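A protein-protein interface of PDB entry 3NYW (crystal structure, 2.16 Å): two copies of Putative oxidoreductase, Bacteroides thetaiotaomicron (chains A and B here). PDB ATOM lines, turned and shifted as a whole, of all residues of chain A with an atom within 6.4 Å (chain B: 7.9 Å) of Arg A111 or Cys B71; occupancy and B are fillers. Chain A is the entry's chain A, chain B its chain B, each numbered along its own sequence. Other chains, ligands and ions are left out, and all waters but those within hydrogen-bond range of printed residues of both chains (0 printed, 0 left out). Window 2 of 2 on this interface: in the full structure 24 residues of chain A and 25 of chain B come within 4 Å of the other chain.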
ATOM      1  N   PRO A 106      12.410 -25.740  -1.154  1.00  0.00           N
ATOM      2  CA  PRO A 106      13.484 -25.205  -0.307  1.00  0.00           C
ATOM      3  C   PRO A 106      13.053 -24.989   1.149  1.00  0.00           C
ATOM      4  O   PRO A 106      13.855 -25.154   2.068  1.00  0.00           O
ATOM      5  CB  PRO A 106      13.847 -23.898  -1.002  1.00  0.00           C
ATOM      6  CG  PRO A 106      13.610 -24.224  -2.435  1.00  0.00           C
ATOM      7  CD  PRO A 106      12.274 -24.930  -2.377  1.00  0.00           C
ATOM      8  N   VAL A 107      11.794 -24.616   1.359  1.00  0.00           N
ATOM      9  CA  VAL A 107      11.304 -24.401   2.712  1.00  0.00           C
ATOM     10  C   VAL A 107      11.405 -25.720   3.468  1.00  0.00           C
ATOM     11  O   VAL A 107      11.575 -25.739   4.691  1.00  0.00           O
ATOM     12  CB  VAL A 107       9.837 -23.922   2.725  1.00  0.00           C
ATOM     13  CG1 VAL A 107       9.332 -23.839   4.150  1.00  0.00           C
ATOM     14  CG2 VAL A 107       9.730 -22.559   2.074  1.00  0.00           C
ATOM     15  N   ASP A 108      11.304 -26.823   2.731  1.00  0.00           N
ATOM     16  CA  ASP A 108      11.397 -28.142   3.341  1.00  0.00           C
ATOM     17  C   ASP A 108      12.865 -28.486   3.550  1.00  0.00           C
ATOM     18  O   ASP A 108      13.217 -29.147   4.524  1.00  0.00           O
ATOM     19  CB  ASP A 108      10.709 -29.202   2.469  1.00  0.00           C
ATOM     20  CG  ASP A 108       9.206 -28.973   2.345  1.00  0.00           C
ATOM     21  OD1 ASP A 108       8.550 -28.712   3.381  1.00  0.00           O
ATOM     22  OD2 ASP A 108       8.680 -29.057   1.214  1.00  0.00           O
ATOM     23  N   ASN A 109      13.721 -28.036   2.637  1.00  0.00           N
ATOM     24  CA  ASN A 109      15.153 -28.278   2.772  1.00  0.00           C
ATOM     25  C   ASN A 109      15.649 -27.494   3.971  1.00  0.00           C
ATOM     26  O   ASN A 109      16.537 -27.942   4.690  1.00  0.00           O
ATOM     27  CB  ASN A 109      15.905 -27.826   1.525  1.00  0.00           C
ATOM     28  CG  ASN A 109      15.669 -28.740   0.354  1.00  0.00           C
ATOM     29  OD1 ASN A 109      15.845 -29.950   0.466  1.00  0.00           O
ATOM     30  ND2 ASN A 109      15.269 -28.173  -0.780  1.00  0.00           N
ATOM     31  N   PHE A 110      15.067 -26.317   4.184  1.00  0.00           N
ATOM     32  CA  PHE A 110      15.446 -25.484   5.316  1.00  0.00           C
ATOM     33  C   PHE A 110      15.062 -26.204   6.610  1.00  0.00           C
ATOM     34  O   PHE A 110      15.817 -26.199   7.573  1.00  0.00           O
ATOM     35  CB  PHE A 110      14.762 -24.110   5.226  1.00  0.00           C
ATOM     36  CG  PHE A 110      15.280 -23.100   6.224  1.00  0.00           C
ATOM     37  CD1 PHE A 110      16.623 -23.086   6.591  1.00  0.00           C
ATOM     38  CD2 PHE A 110      14.430 -22.152   6.782  1.00  0.00           C
ATOM     39  CE1 PHE A 110      17.112 -22.141   7.503  1.00  0.00           C
ATOM     40  CE2 PHE A 110      14.909 -21.206   7.691  1.00  0.00           C
ATOM     41  CZ  PHE A 110      16.255 -21.204   8.052  1.00  0.00           C
ATOM     42  N   ARG A 111      13.891 -26.832   6.629  1.00  0.00           N
ATOM     43  CA  ARG A 111      13.463 -27.566   7.814  1.00  0.00           C
ATOM     44  C   ARG A 111      14.469 -28.649   8.143  1.00  0.00           C
ATOM     45  O   ARG A 111      14.983 -28.711   9.257  1.00  0.00           O
ATOM     46  CB  ARG A 111      12.108 -28.238   7.608  1.00  0.00           C
ATOM     47  CG  ARG A 111      10.917 -27.356   7.825  1.00  0.00           C
ATOM     48  CD  ARG A 111       9.715 -28.198   8.211  1.00  0.00           C
ATOM     49  NE  ARG A 111       8.480 -27.425   8.159  1.00  0.00           N
ATOM     50  CZ  ARG A 111       7.969 -26.918   7.043  1.00  0.00           C
ATOM     51  NH1 ARG A 111       8.588 -27.108   5.885  1.00  0.00           N
ATOM     52  NH2 ARG A 111       6.843 -26.216   7.083  1.00  0.00           N
ATOM     53  N   LYS A 112      14.742 -29.508   7.165  1.00  0.00           N
ATOM     54  CA  LYS A 112      15.679 -30.606   7.359  1.00  0.00           C
ATOM     55  C   LYS A 112      17.066 -30.129   7.771  1.00  0.00           C
ATOM     56  O   LYS A 112      17.711 -30.740   8.618  1.00  0.00           O
ATOM     57  CB  LYS A 112      15.787 -31.455   6.087  1.00  0.00           C
ATOM     58  CG  LYS A 112      16.619 -32.720   6.288  1.00  0.00           C
ATOM     59  CD  LYS A 112      16.645 -33.619   5.056  1.00  0.00           C
ATOM     60  CE  LYS A 112      17.444 -33.000   3.920  1.00  0.00           C
ATOM     61  NZ  LYS A 112      17.639 -33.968   2.802  1.00  0.00           N
ATOM     62  N   ILE A 113      17.531 -29.044   7.167  1.00  0.00           N
ATOM     63  CA  ILE A 113      18.844 -28.515   7.502  1.00  0.00           C
ATOM     64  C   ILE A 113      18.867 -28.028   8.953  1.00  0.00           C
ATOM     65  O   ILE A 113      19.823 -28.264   9.677  1.00  0.00           O
ATOM     66  CB  ILE A 113      19.227 -27.371   6.545  1.00  0.00           C
ATOM     67  CG1 ILE A 113      19.482 -27.950   5.152  1.00  0.00           C
ATOM     68  CG2 ILE A 113      20.447 -26.634   7.056  1.00  0.00           C
ATOM     69  CD1 ILE A 113      19.660 -26.902   4.077  1.00  0.00           C
ATOM     70  N   MET A 114      17.800 -27.363   9.372  1.00  0.00           N
ATOM     71  CA  MET A 114      17.696 -26.865  10.738  1.00  0.00           C
ATOM     72  C   MET A 114      17.614 -28.040  11.723  1.00  0.00           C
ATOM     73  O   MET A 114      18.219 -28.018  12.796  1.00  0.00           O
ATOM     74  CB  MET A 114      16.453 -25.977  10.863  1.00  0.00           C
ATOM     75  CG  MET A 114      16.352 -25.182  12.158  1.00  0.00           C
ATOM     76  SD  MET A 114      17.807 -23.907  12.392  1.00  0.00           S
ATOM     77  CE  MET A 114      18.084 -23.378  10.545  1.00  0.00           C
ATOM     78  N   GLU A 115      16.865 -29.069  11.343  1.00  0.00           N
ATOM     79  CA  GLU A 115      16.693 -30.256  12.176  1.00  0.00           C
ATOM     80  C   GLU A 115      18.010 -30.988  12.420  1.00  0.00           C
ATOM     81  O   GLU A 115      18.337 -31.337  13.558  1.00  0.00           O
ATOM     82  CB  GLU A 115      15.712 -31.222  11.511  1.00  0.00           C
ATOM     83  CG  GLU A 115      15.551 -32.568  12.215  1.00  0.00           C
ATOM     84  CD  GLU A 115      14.842 -32.458  13.558  1.00  0.00           C
ATOM     85  OE1 GLU A 115      13.834 -31.721  13.634  1.00  0.00           O
ATOM     86  OE2 GLU A 115      15.283 -33.115  14.525  1.00  0.00           O
ATOM     87  N   ILE A 116      18.757 -31.219  11.346  1.00  0.00           N
ATOM     88  CA  ILE A 116      20.024 -31.932  11.427  1.00  0.00           C
ATOM     89  C   ILE A 116      21.170 -31.173  12.107  1.00  0.00           C
ATOM     90  O   ILE A 116      22.028 -31.788  12.745  1.00  0.00           O
ATOM     91  CB  ILE A 116      20.498 -32.352  10.023  1.00  0.00           C
ATOM     92  CG1 ILE A 116      19.453 -33.250   9.367  1.00  0.00           C
ATOM     93  CG2 ILE A 116      21.832 -33.090  10.119  1.00  0.00           C
ATOM     94  CD1 ILE A 116      19.796 -33.619   7.943  1.00  0.00           C
ATOM     95  N   ILE A 119      18.554 -28.474  15.920  1.00  0.00           N
ATOM     96  CA  ILE A 119      17.731 -29.248  16.841  1.00  0.00           C
ATOM     97  C   ILE A 119      18.532 -30.426  17.388  1.00  0.00           C
ATOM     98  O   ILE A 119      18.495 -30.709  18.583  1.00  0.00           O
ATOM     99  CB  ILE A 119      16.455 -29.779  16.149  1.00  0.00           C
ATOM    100  CG1 ILE A 119      15.689 -28.618  15.517  1.00  0.00           C
ATOM    101  CG2 ILE A 119      15.552 -30.469  17.165  1.00  0.00           C
ATOM    102  CD1 ILE A 119      15.264 -27.580  16.514  1.00  0.00           C
ATOM    103  N   LEU B  66      -4.411 -14.984   7.793  1.00  0.00           N
ATOM    104  CA  LEU B  66      -3.488 -16.050   7.449  1.00  0.00           C
ATOM    105  C   LEU B  66      -2.461 -16.410   8.508  1.00  0.00           C
ATOM    106  O   LEU B  66      -1.755 -15.553   9.031  1.00  0.00           O
ATOM    107  CB  LEU B  66      -2.750 -15.678   6.164  1.00  0.00           C
ATOM    108  CG  LEU B  66      -1.560 -16.563   5.797  1.00  0.00           C
ATOM    109  CD1 LEU B  66      -2.052 -17.950   5.388  1.00  0.00           C
ATOM    110  CD2 LEU B  66      -0.775 -15.904   4.669  1.00  0.00           C
ATOM    111  N   ASP B  67      -2.380 -17.700   8.804  1.00  0.00           N
ATOM    112  CA  ASP B  67      -1.409 -18.210   9.760  1.00  0.00           C
ATOM    113  C   ASP B  67      -0.174 -18.555   8.928  1.00  0.00           C
ATOM    114  O   ASP B  67      -0.099 -19.644   8.349  1.00  0.00           O
ATOM    115  CB  ASP B  67      -1.961 -19.466  10.439  1.00  0.00           C
ATOM    116  CG  ASP B  67      -0.915 -20.197  11.254  1.00  0.00           C
ATOM    117  OD1 ASP B  67       0.190 -19.651  11.443  1.00  0.00           O
ATOM    118  OD2 ASP B  67      -1.206 -21.321  11.712  1.00  0.00           O
ATOM    119  N   ILE B  68       0.785 -17.631   8.863  1.00  0.00           N
ATOM    120  CA  ILE B  68       1.989 -17.843   8.060  1.00  0.00           C
ATOM    121  C   ILE B  68       2.700 -19.164   8.327  1.00  0.00           C
ATOM    122  O   ILE B  68       3.582 -19.564   7.566  1.00  0.00           O
ATOM    123  CB  ILE B  68       2.988 -16.668   8.203  1.00  0.00           C
ATOM    124  CG1 ILE B  68       3.425 -16.504   9.659  1.00  0.00           C
ATOM    125  CG2 ILE B  68       2.334 -15.386   7.701  1.00  0.00           C
ATOM    126  CD1 ILE B  68       4.465 -15.421   9.859  1.00  0.00           C
ATOM    127  N   THR B  69       2.305 -19.846   9.398  1.00  0.00           N
ATOM    128  CA  THR B  69       2.878 -21.145   9.734  1.00  0.00           C
ATOM    129  C   THR B  69       2.569 -22.122   8.594  1.00  0.00           C
ATOM    130  O   THR B  69       3.337 -23.047   8.323  1.00  0.00           O
ATOM    131  CB  THR B  69       2.289 -21.682  11.052  1.00  0.00           C
ATOM    132  OG1 THR B  69       2.835 -20.938  12.146  1.00  0.00           O
ATOM    133  CG2 THR B  69       2.609 -23.155  11.234  1.00  0.00           C
ATOM    134  N   ASP B  70       1.434 -21.908   7.933  1.00  0.00           N
ATOM    135  CA  ASP B  70       1.025 -22.731   6.802  1.00  0.00           C
ATOM    136  C   ASP B  70       1.707 -22.121   5.575  1.00  0.00           C
ATOM    137  O   ASP B  70       1.094 -21.363   4.815  1.00  0.00           O
ATOM    138  CB  ASP B  70      -0.493 -22.679   6.640  1.00  0.00           C
ATOM    139  CG  ASP B  70      -0.997 -23.610   5.558  1.00  0.00           C
ATOM    140  OD1 ASP B  70      -0.169 -24.205   4.839  1.00  0.00           O
ATOM    141  OD2 ASP B  70      -2.228 -23.744   5.423  1.00  0.00           O
ATOM    142  N   CYS B  71       2.982 -22.458   5.401  1.00  0.00           N
ATOM    143  CA  CYS B  71       3.803 -21.939   4.312  1.00  0.00           C
ATOM    144  C   CYS B  71       3.173 -21.939   2.919  1.00  0.00           C
ATOM    145  O   CYS B  71       3.027 -20.885   2.301  1.00  0.00           O
ATOM    146  CB  CYS B  71       5.136 -22.693   4.275  1.00  0.00           C
ATOM    147  SG  CYS B  71       6.086 -22.611   5.825  1.00  0.00           S
ATOM    148  N   THR B  72       2.807 -23.115   2.424  1.00  0.00           N
ATOM    149  CA  THR B  72       2.209 -23.234   1.097  1.00  0.00           C
ATOM    150  C   THR B  72       1.014 -22.313   0.879  1.00  0.00           C
ATOM    151  O   THR B  72       0.894 -21.686  -0.170  1.00  0.00           O
ATOM    152  CB  THR B  72       1.772 -24.682   0.818  1.00  0.00           C
ATOM    153  OG1 THR B  72       2.925 -25.534   0.833  1.00  0.00           O
ATOM    154  CG2 THR B  72       1.081 -24.782  -0.535  1.00  0.00           C
ATOM    155  N   LYS B  73       0.124 -22.244   1.865  1.00  0.00           N
ATOM    156  CA  LYS B  73      -1.056 -21.389   1.769  1.00  0.00           C
ATOM    157  C   LYS B  73      -0.636 -19.925   1.734  1.00  0.00           C
ATOM    158  O   LYS B  73      -1.186 -19.129   0.977  1.00  0.00           O
ATOM    159  CB  LYS B  73      -1.983 -21.622   2.963  1.00  0.00           C
ATOM    160  CG  LYS B  73      -3.279 -20.828   2.897  1.00  0.00           C
ATOM    161  CD  LYS B  73      -4.052 -20.916   4.206  1.00  0.00           C
ATOM    162  CE  LYS B  73      -5.361 -20.139   4.145  1.00  0.00           C
ATOM    163  NZ  LYS B  73      -6.301 -20.713   3.140  1.00  0.00           N
ATOM    164  N   ALA B  74       0.343 -19.580   2.563  1.00  0.00           N
ATOM    165  CA  ALA B  74       0.848 -18.216   2.638  1.00  0.00           C
ATOM    166  C   ALA B  74       1.410 -17.785   1.292  1.00  0.00           C
ATOM    167  O   ALA B  74       1.112 -16.707   0.797  1.00  0.00           O
ATOM    168  CB  ALA B  74       1.928 -18.121   3.710  1.00  0.00           C
ATOM    169  N   ASP B  75       2.229 -18.640   0.697  1.00  0.00           N
ATOM    170  CA  ASP B  75       2.820 -18.322  -0.589  1.00  0.00           C
ATOM    171  C   ASP B  75       1.737 -18.129  -1.644  1.00  0.00           C
ATOM    172  O   ASP B  75       1.819 -17.226  -2.472  1.00  0.00           O
ATOM    173  CB  ASP B  75       3.791 -19.421  -1.015  1.00  0.00           C
ATOM    174  CG  ASP B  75       4.326 -19.206  -2.415  1.00  0.00           C
ATOM    175  OD1 ASP B  75       3.605 -19.543  -3.375  1.00  0.00           O
ATOM    176  OD2 ASP B  75       5.453 -18.688  -2.560  1.00  0.00           O
ATOM    177  N   THR B  76       0.719 -18.978  -1.607  1.00  0.00           N
ATOM    178  CA  THR B  76      -0.382 -18.879  -2.558  1.00  0.00           C
ATOM    179  C   THR B  76      -1.131 -17.556  -2.366  1.00  0.00           C
ATOM    180  O   THR B  76      -1.305 -16.785  -3.310  1.00  0.00           O
ATOM    181  CB  THR B  76      -1.380 -20.051  -2.385  1.00  0.00           C
ATOM    182  OG1 THR B  76      -0.751 -21.280  -2.776  1.00  0.00           O
ATOM    183  CG2 THR B  76      -2.626 -19.827  -3.241  1.00  0.00           C
ATOM    184  N   GLU B  77      -1.566 -17.296  -1.138  1.00  0.00           N
ATOM    185  CA  GLU B  77      -2.296 -16.073  -0.837  1.00  0.00           C
ATOM    186  C   GLU B  77      -1.541 -14.819  -1.260  1.00  0.00           C
ATOM    187  O   GLU B  77      -2.142 -13.878  -1.772  1.00  0.00           O
ATOM    188  CB  GLU B  77      -2.607 -15.993   0.657  1.00  0.00           C
ATOM    189  CG  GLU B  77      -3.631 -16.998   1.137  1.00  0.00           C
ATOM    190  CD  GLU B  77      -4.943 -16.866   0.401  1.00  0.00           C
ATOM    191  OE1 GLU B  77      -5.444 -15.729   0.285  1.00  0.00           O
ATOM    192  OE2 GLU B  77      -5.482 -17.896  -0.059  1.00  0.00           O
ATOM    193  N   ILE B  78      -0.229 -14.802  -1.052  1.00  0.00           N
ATOM    194  CA  ILE B  78       0.561 -13.631  -1.405  1.00  0.00           C
ATOM    195  C   ILE B  78       0.706 -13.466  -2.915  1.00  0.00           C
ATOM    196  O   ILE B  78       0.829 -12.352  -3.426  1.00  0.00           O
ATOM    197  CB  ILE B  78       1.965 -13.680  -0.739  1.00  0.00           C
ATOM    198  CG1 ILE B  78       1.808 -13.624   0.788  1.00  0.00           C
ATOM    199  CG2 ILE B  78       2.822 -12.511  -1.223  1.00  0.00           C
ATOM    200  CD1 ILE B  78       3.103 -13.440   1.550  1.00  0.00           C
ATOM    201  N   ARG B 111      11.859 -27.414  18.428  1.00  0.00           N
ATOM    202  CA  ARG B 111      11.612 -27.664  17.014  1.00  0.00           C
ATOM    203  C   ARG B 111      10.409 -26.846  16.552  1.00  0.00           C
ATOM    204  O   ARG B 111      10.395 -26.313  15.441  1.00  0.00           O
ATOM    205  CB  ARG B 111      11.338 -29.150  16.796  1.00  0.00           C
ATOM    206  CG  ARG B 111      11.866 -29.720  15.488  1.00  0.00           C
ATOM    207  CD  ARG B 111      11.257 -31.094  15.231  1.00  0.00           C
ATOM    208  NE  ARG B 111      11.196 -31.901  16.450  1.00  0.00           N
ATOM    209  CZ  ARG B 111      12.083 -32.828  16.791  1.00  0.00           C
ATOM    210  NH1 ARG B 111      13.114 -33.084  16.000  1.00  0.00           N
ATOM    211  NH2 ARG B 111      11.932 -33.498  17.926  1.00  0.00           N
ATOM    212  N   MET B 114      11.182 -23.029  16.354  1.00  0.00           N
ATOM    213  CA  MET B 114      11.964 -22.736  15.148  1.00  0.00           C
ATOM    214  C   MET B 114      11.058 -22.681  13.923  1.00  0.00           C
ATOM    215  O   MET B 114      11.192 -21.804  13.071  1.00  0.00           O
ATOM    216  CB  MET B 114      13.024 -23.812  14.925  1.00  0.00           C
ATOM    217  CG  MET B 114      14.331 -23.559  15.637  1.00  0.00           C
ATOM    218  SD  MET B 114      15.227 -22.005  14.908  1.00  0.00           S
ATOM    219  CE  MET B 114      16.400 -21.630  16.409  1.00  0.00           C
ATOM    220  N   GLU B 115      10.143 -23.640  13.844  1.00  0.00           N
ATOM    221  CA  GLU B 115       9.194 -23.726  12.742  1.00  0.00           C
ATOM    222  C   GLU B 115       8.371 -22.440  12.670  1.00  0.00           C
ATOM    223  O   GLU B 115       8.361 -21.746  11.647  1.00  0.00           O
ATOM    224  CB  GLU B 115       8.275 -24.936  12.957  1.00  0.00           C
ATOM    225  CG  GLU B 115       7.228 -25.173  11.875  1.00  0.00           C
ATOM    226  CD  GLU B 115       7.829 -25.288  10.488  1.00  0.00           C
ATOM    227  OE1 GLU B 115       8.960 -25.808  10.366  1.00  0.00           O
ATOM    228  OE2 GLU B 115       7.163 -24.868   9.521  1.00  0.00           O
ATOM    229  N   ILE B 116       7.704 -22.116  13.772  1.00  0.00           N
ATOM    230  CA  ILE B 116       6.869 -20.927  13.851  1.00  0.00           C
ATOM    231  C   ILE B 116       7.595 -19.601  13.619  1.00  0.00           C
ATOM    232  O   ILE B 116       7.102 -18.732  12.899  1.00  0.00           O
ATOM    233  CB  ILE B 116       6.176 -20.838  15.224  1.00  0.00           C
ATOM    234  CG1 ILE B 116       5.252 -22.042  15.414  1.00  0.00           C
ATOM    235  CG2 ILE B 116       5.402 -19.520  15.338  1.00  0.00           C
ATOM    236  CD1 ILE B 116       4.493 -22.047  16.729  1.00  0.00           C
ATOM    237  N   VAL B 118      11.229 -19.077  12.633  1.00  0.00           N
ATOM    238  CA  VAL B 118      12.226 -18.970  11.576  1.00  0.00           C
ATOM    239  C   VAL B 118      11.830 -19.627  10.261  1.00  0.00           C
ATOM    240  O   VAL B 118      11.987 -19.028   9.201  1.00  0.00           O
ATOM    241  CB  VAL B 118      13.574 -19.554  12.045  1.00  0.00           C
ATOM    242  CG1 VAL B 118      14.631 -19.352  10.982  1.00  0.00           C
ATOM    243  CG2 VAL B 118      13.992 -18.892  13.344  1.00  0.00           C
ATOM    244  N   ILE B 119      11.333 -20.858  10.320  1.00  0.00           N
ATOM    245  CA  ILE B 119      10.926 -21.562   9.106  1.00  0.00           C
ATOM    246  C   ILE B 119       9.791 -20.818   8.424  1.00  0.00           C
ATOM    247  O   ILE B 119       9.767 -20.678   7.201  1.00  0.00           O
ATOM    248  CB  ILE B 119      10.446 -22.994   9.411  1.00  0.00           C
ATOM    249  CG1 ILE B 119      11.617 -23.838   9.916  1.00  0.00           C
ATOM    250  CG2 ILE B 119       9.836 -23.614   8.165  1.00  0.00           C
ATOM    251  CD1 ILE B 119      12.737 -23.986   8.915  1.00  0.00           C
ATOM    252  N   ALA B 120       8.850 -20.338   9.228  1.00  0.00           N
ATOM    253  CA  ALA B 120       7.707 -19.610   8.702  1.00  0.00           C
ATOM    254  C   ALA B 120       8.147 -18.306   8.046  1.00  0.00           C
ATOM    255  O   ALA B 120       7.740 -18.005   6.926  1.00  0.00           O
ATOM    256  CB  ALA B 120       6.706 -19.328   9.821  1.00  0.00           C
ATOM    257  N   GLN B 121       8.978 -17.534   8.742  1.00  0.00           N
ATOM    258  CA  GLN B 121       9.449 -16.267   8.205  1.00  0.00           C
ATOM    259  C   GLN B 121      10.232 -16.484   6.922  1.00  0.00           C
ATOM    260  O   GLN B 121      10.076 -15.736   5.965  1.00  0.00           O
ATOM    261  CB  GLN B 121      10.308 -15.532   9.228  1.00  0.00           C
ATOM    262  CG  GLN B 121      10.891 -14.236   8.696  1.00  0.00           C
ATOM    263  CD  GLN B 121      10.883 -13.118   9.724  1.00  0.00           C
ATOM    264  OE1 GLN B 121      11.597 -12.121   9.579  1.00  0.00           O
ATOM    265  NE2 GLN B 121      10.064 -13.271  10.764  1.00  0.00           N
ATOM    266  N   TYR B 122      11.075 -17.510   6.905  1.00  0.00           N
ATOM    267  CA  TYR B 122      11.849 -17.824   5.711  1.00  0.00           C
ATOM    268  C   TYR B 122      10.870 -17.999   4.547  1.00  0.00           C
ATOM    269  O   TYR B 122      11.106 -17.514   3.444  1.00  0.00           O
ATOM    270  CB  TYR B 122      12.640 -19.118   5.910  1.00  0.00           C
ATOM    271  CG  TYR B 122      13.250 -19.657   4.637  1.00  0.00           C
ATOM    272  CD1 TYR B 122      14.457 -19.166   4.156  1.00  0.00           C
ATOM    273  CD2 TYR B 122      12.597 -20.641   3.896  1.00  0.00           C
ATOM    274  CE1 TYR B 122      15.006 -19.641   2.969  1.00  0.00           C
ATOM    275  CE2 TYR B 122      13.132 -21.122   2.706  1.00  0.00           C
ATOM    276  CZ  TYR B 122      14.338 -20.618   2.247  1.00  0.00           C
ATOM    277  OH  TYR B 122      14.870 -21.082   1.063  1.00  0.00           O
ATOM    278  N   GLY B 123       9.774 -18.705   4.810  1.00  0.00           N
ATOM    279  CA  GLY B 123       8.766 -18.938   3.790  1.00  0.00           C
ATOM    280  C   GLY B 123       8.189 -17.649   3.235  1.00  0.00           C
ATOM    281  O   GLY B 123       8.032 -17.499   2.020  1.00  0.00           O
ATOM    282  N   ILE B 124       7.869 -16.715   4.122  1.00  0.00           N
ATOM    283  CA  ILE B 124       7.331 -15.435   3.688  1.00  0.00           C
ATOM    284  C   ILE B 124       8.357 -14.704   2.824  1.00  0.00           C
ATOM    285  O   ILE B 124       8.033 -14.226   1.736  1.00  0.00           O
ATOM    286  CB  ILE B 124       6.994 -14.536   4.884  1.00  0.00           C
ATOM    287  CG1 ILE B 124       5.893 -15.181   5.732  1.00  0.00           C
ATOM    288  CG2 ILE B 124       6.603 -13.158   4.388  1.00  0.00           C
ATOM    289  CD1 ILE B 124       4.534 -15.270   5.038  1.00  0.00           C
ATOM    290  N   THR B 127       8.770 -16.076  -0.756  1.00  0.00           N
ATOM    291  CA  THR B 127       7.713 -15.598  -1.641  1.00  0.00           C
ATOM    292  C   THR B 127       7.916 -14.140  -2.048  1.00  0.00           C
ATOM    293  O   THR B 127       7.980 -13.827  -3.235  1.00  0.00           O
ATOM    294  CB  THR B 127       6.341 -15.722  -0.974  1.00  0.00           C
ATOM    295  OG1 THR B 127       6.111 -17.087  -0.616  1.00  0.00           O
ATOM    296  CG2 THR B 127       5.246 -15.257  -1.915  1.00  0.00           C
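Printed residues of chain B within 4 Å of Val A107: Cys B71 (3.9 Å) and Tyr B122 (3.7 Å).
Printed residues of chain B within 4 Å of Phe A110: Val B118 (3.8 Å), Ile B119 (3.3 Å) and Tyr B122 (3.5 Å).
Arg A111 touches just these residues of chain B: Cys B71 (3.9 Å), Glu B115 (2.8 Å) and Ile B119 (3.8 Å).
Printed residues of chain B within 4 Å of Glu A115: Arg B111 (2.6 Å).
Printed residues of chain A within 4 Å of Cys B71: Val A107 and Arg A111.
Of the printed residues of chain A, Glu B115 touches Arg A111.
The nearest residue of chain B that does not touch Arg A111 is Thr B69 (4.9 Å).
The nearest printed residue of chain A that does not touch Arg B111 is Met A114 (6.9 Å).
Of the 12 printed residues of chain A, 6 touch a printed residue of chain B.
Along chain B the printed residues that touch a printed residue of chain A span positions 71 to 122.
Arg A111 touches Glu B115, and with the chains exchanged Glu A115 touches Arg B111.
Arg A111 touches Ile B119, and with the chains exchanged Ile A119 touches Arg B111.
Of the 11 pairs that touch across the chains among the printed residues, 4 have their exchanged pair printed and touching as well.
The guanidinium group (NH1) of Arg B111 is in salt-bridge range of the side-chain carboxylate (OE2) of Glu A115, 2.6 Å away.
The guanidinium group (NE) of Arg A111 is in salt-bridge range of the side-chain carboxylate (OE1) of Glu B115.
N of Ile B119 sits at hydrogen-bond distance from O of Met B114, at 2.9 Å.
The backbone NH of Ile A119 is in hydrogen-bond range of the backbone carbonyl oxygen of Met A114.
O of Thr B69 is in hydrogen-bond range of SG of Cys B71, 3.7 Å away.
The guanidinium group (NH1) of Arg A111 is in salt-bridge range of the side-chain carboxylate (OD1) of Asp A108 (3.0 Å).
The backbone NH (N) of Ala B120 is in hydrogen-bond range of the backbone carbonyl oxygen (O) of Glu B115 (2.8 Å).
The backbone carbonyl oxygen of Val A107 sits at hydrogen-bond distance from the guanidinium group of Arg A111 (3.5 Å).
Among the printed residues, pairs that only touch across the chains: Pro A106 with Tyr B122 (3.6 Å), Val A107 with Cys B71 (3.9 Å), Val A107 with Tyr B122 (3.7 Å), Phe A110 with Val B118 (3.8 Å), Phe A110 with Ile B119 (3.3 Å), Phe A110 with Tyr B122 (3.5 Å), Arg A111 with Cys B71 (3.9 Å), Arg A111 with Ile B119 (3.8 Å) and Ile A119 with Arg B111 (3.7 Å).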
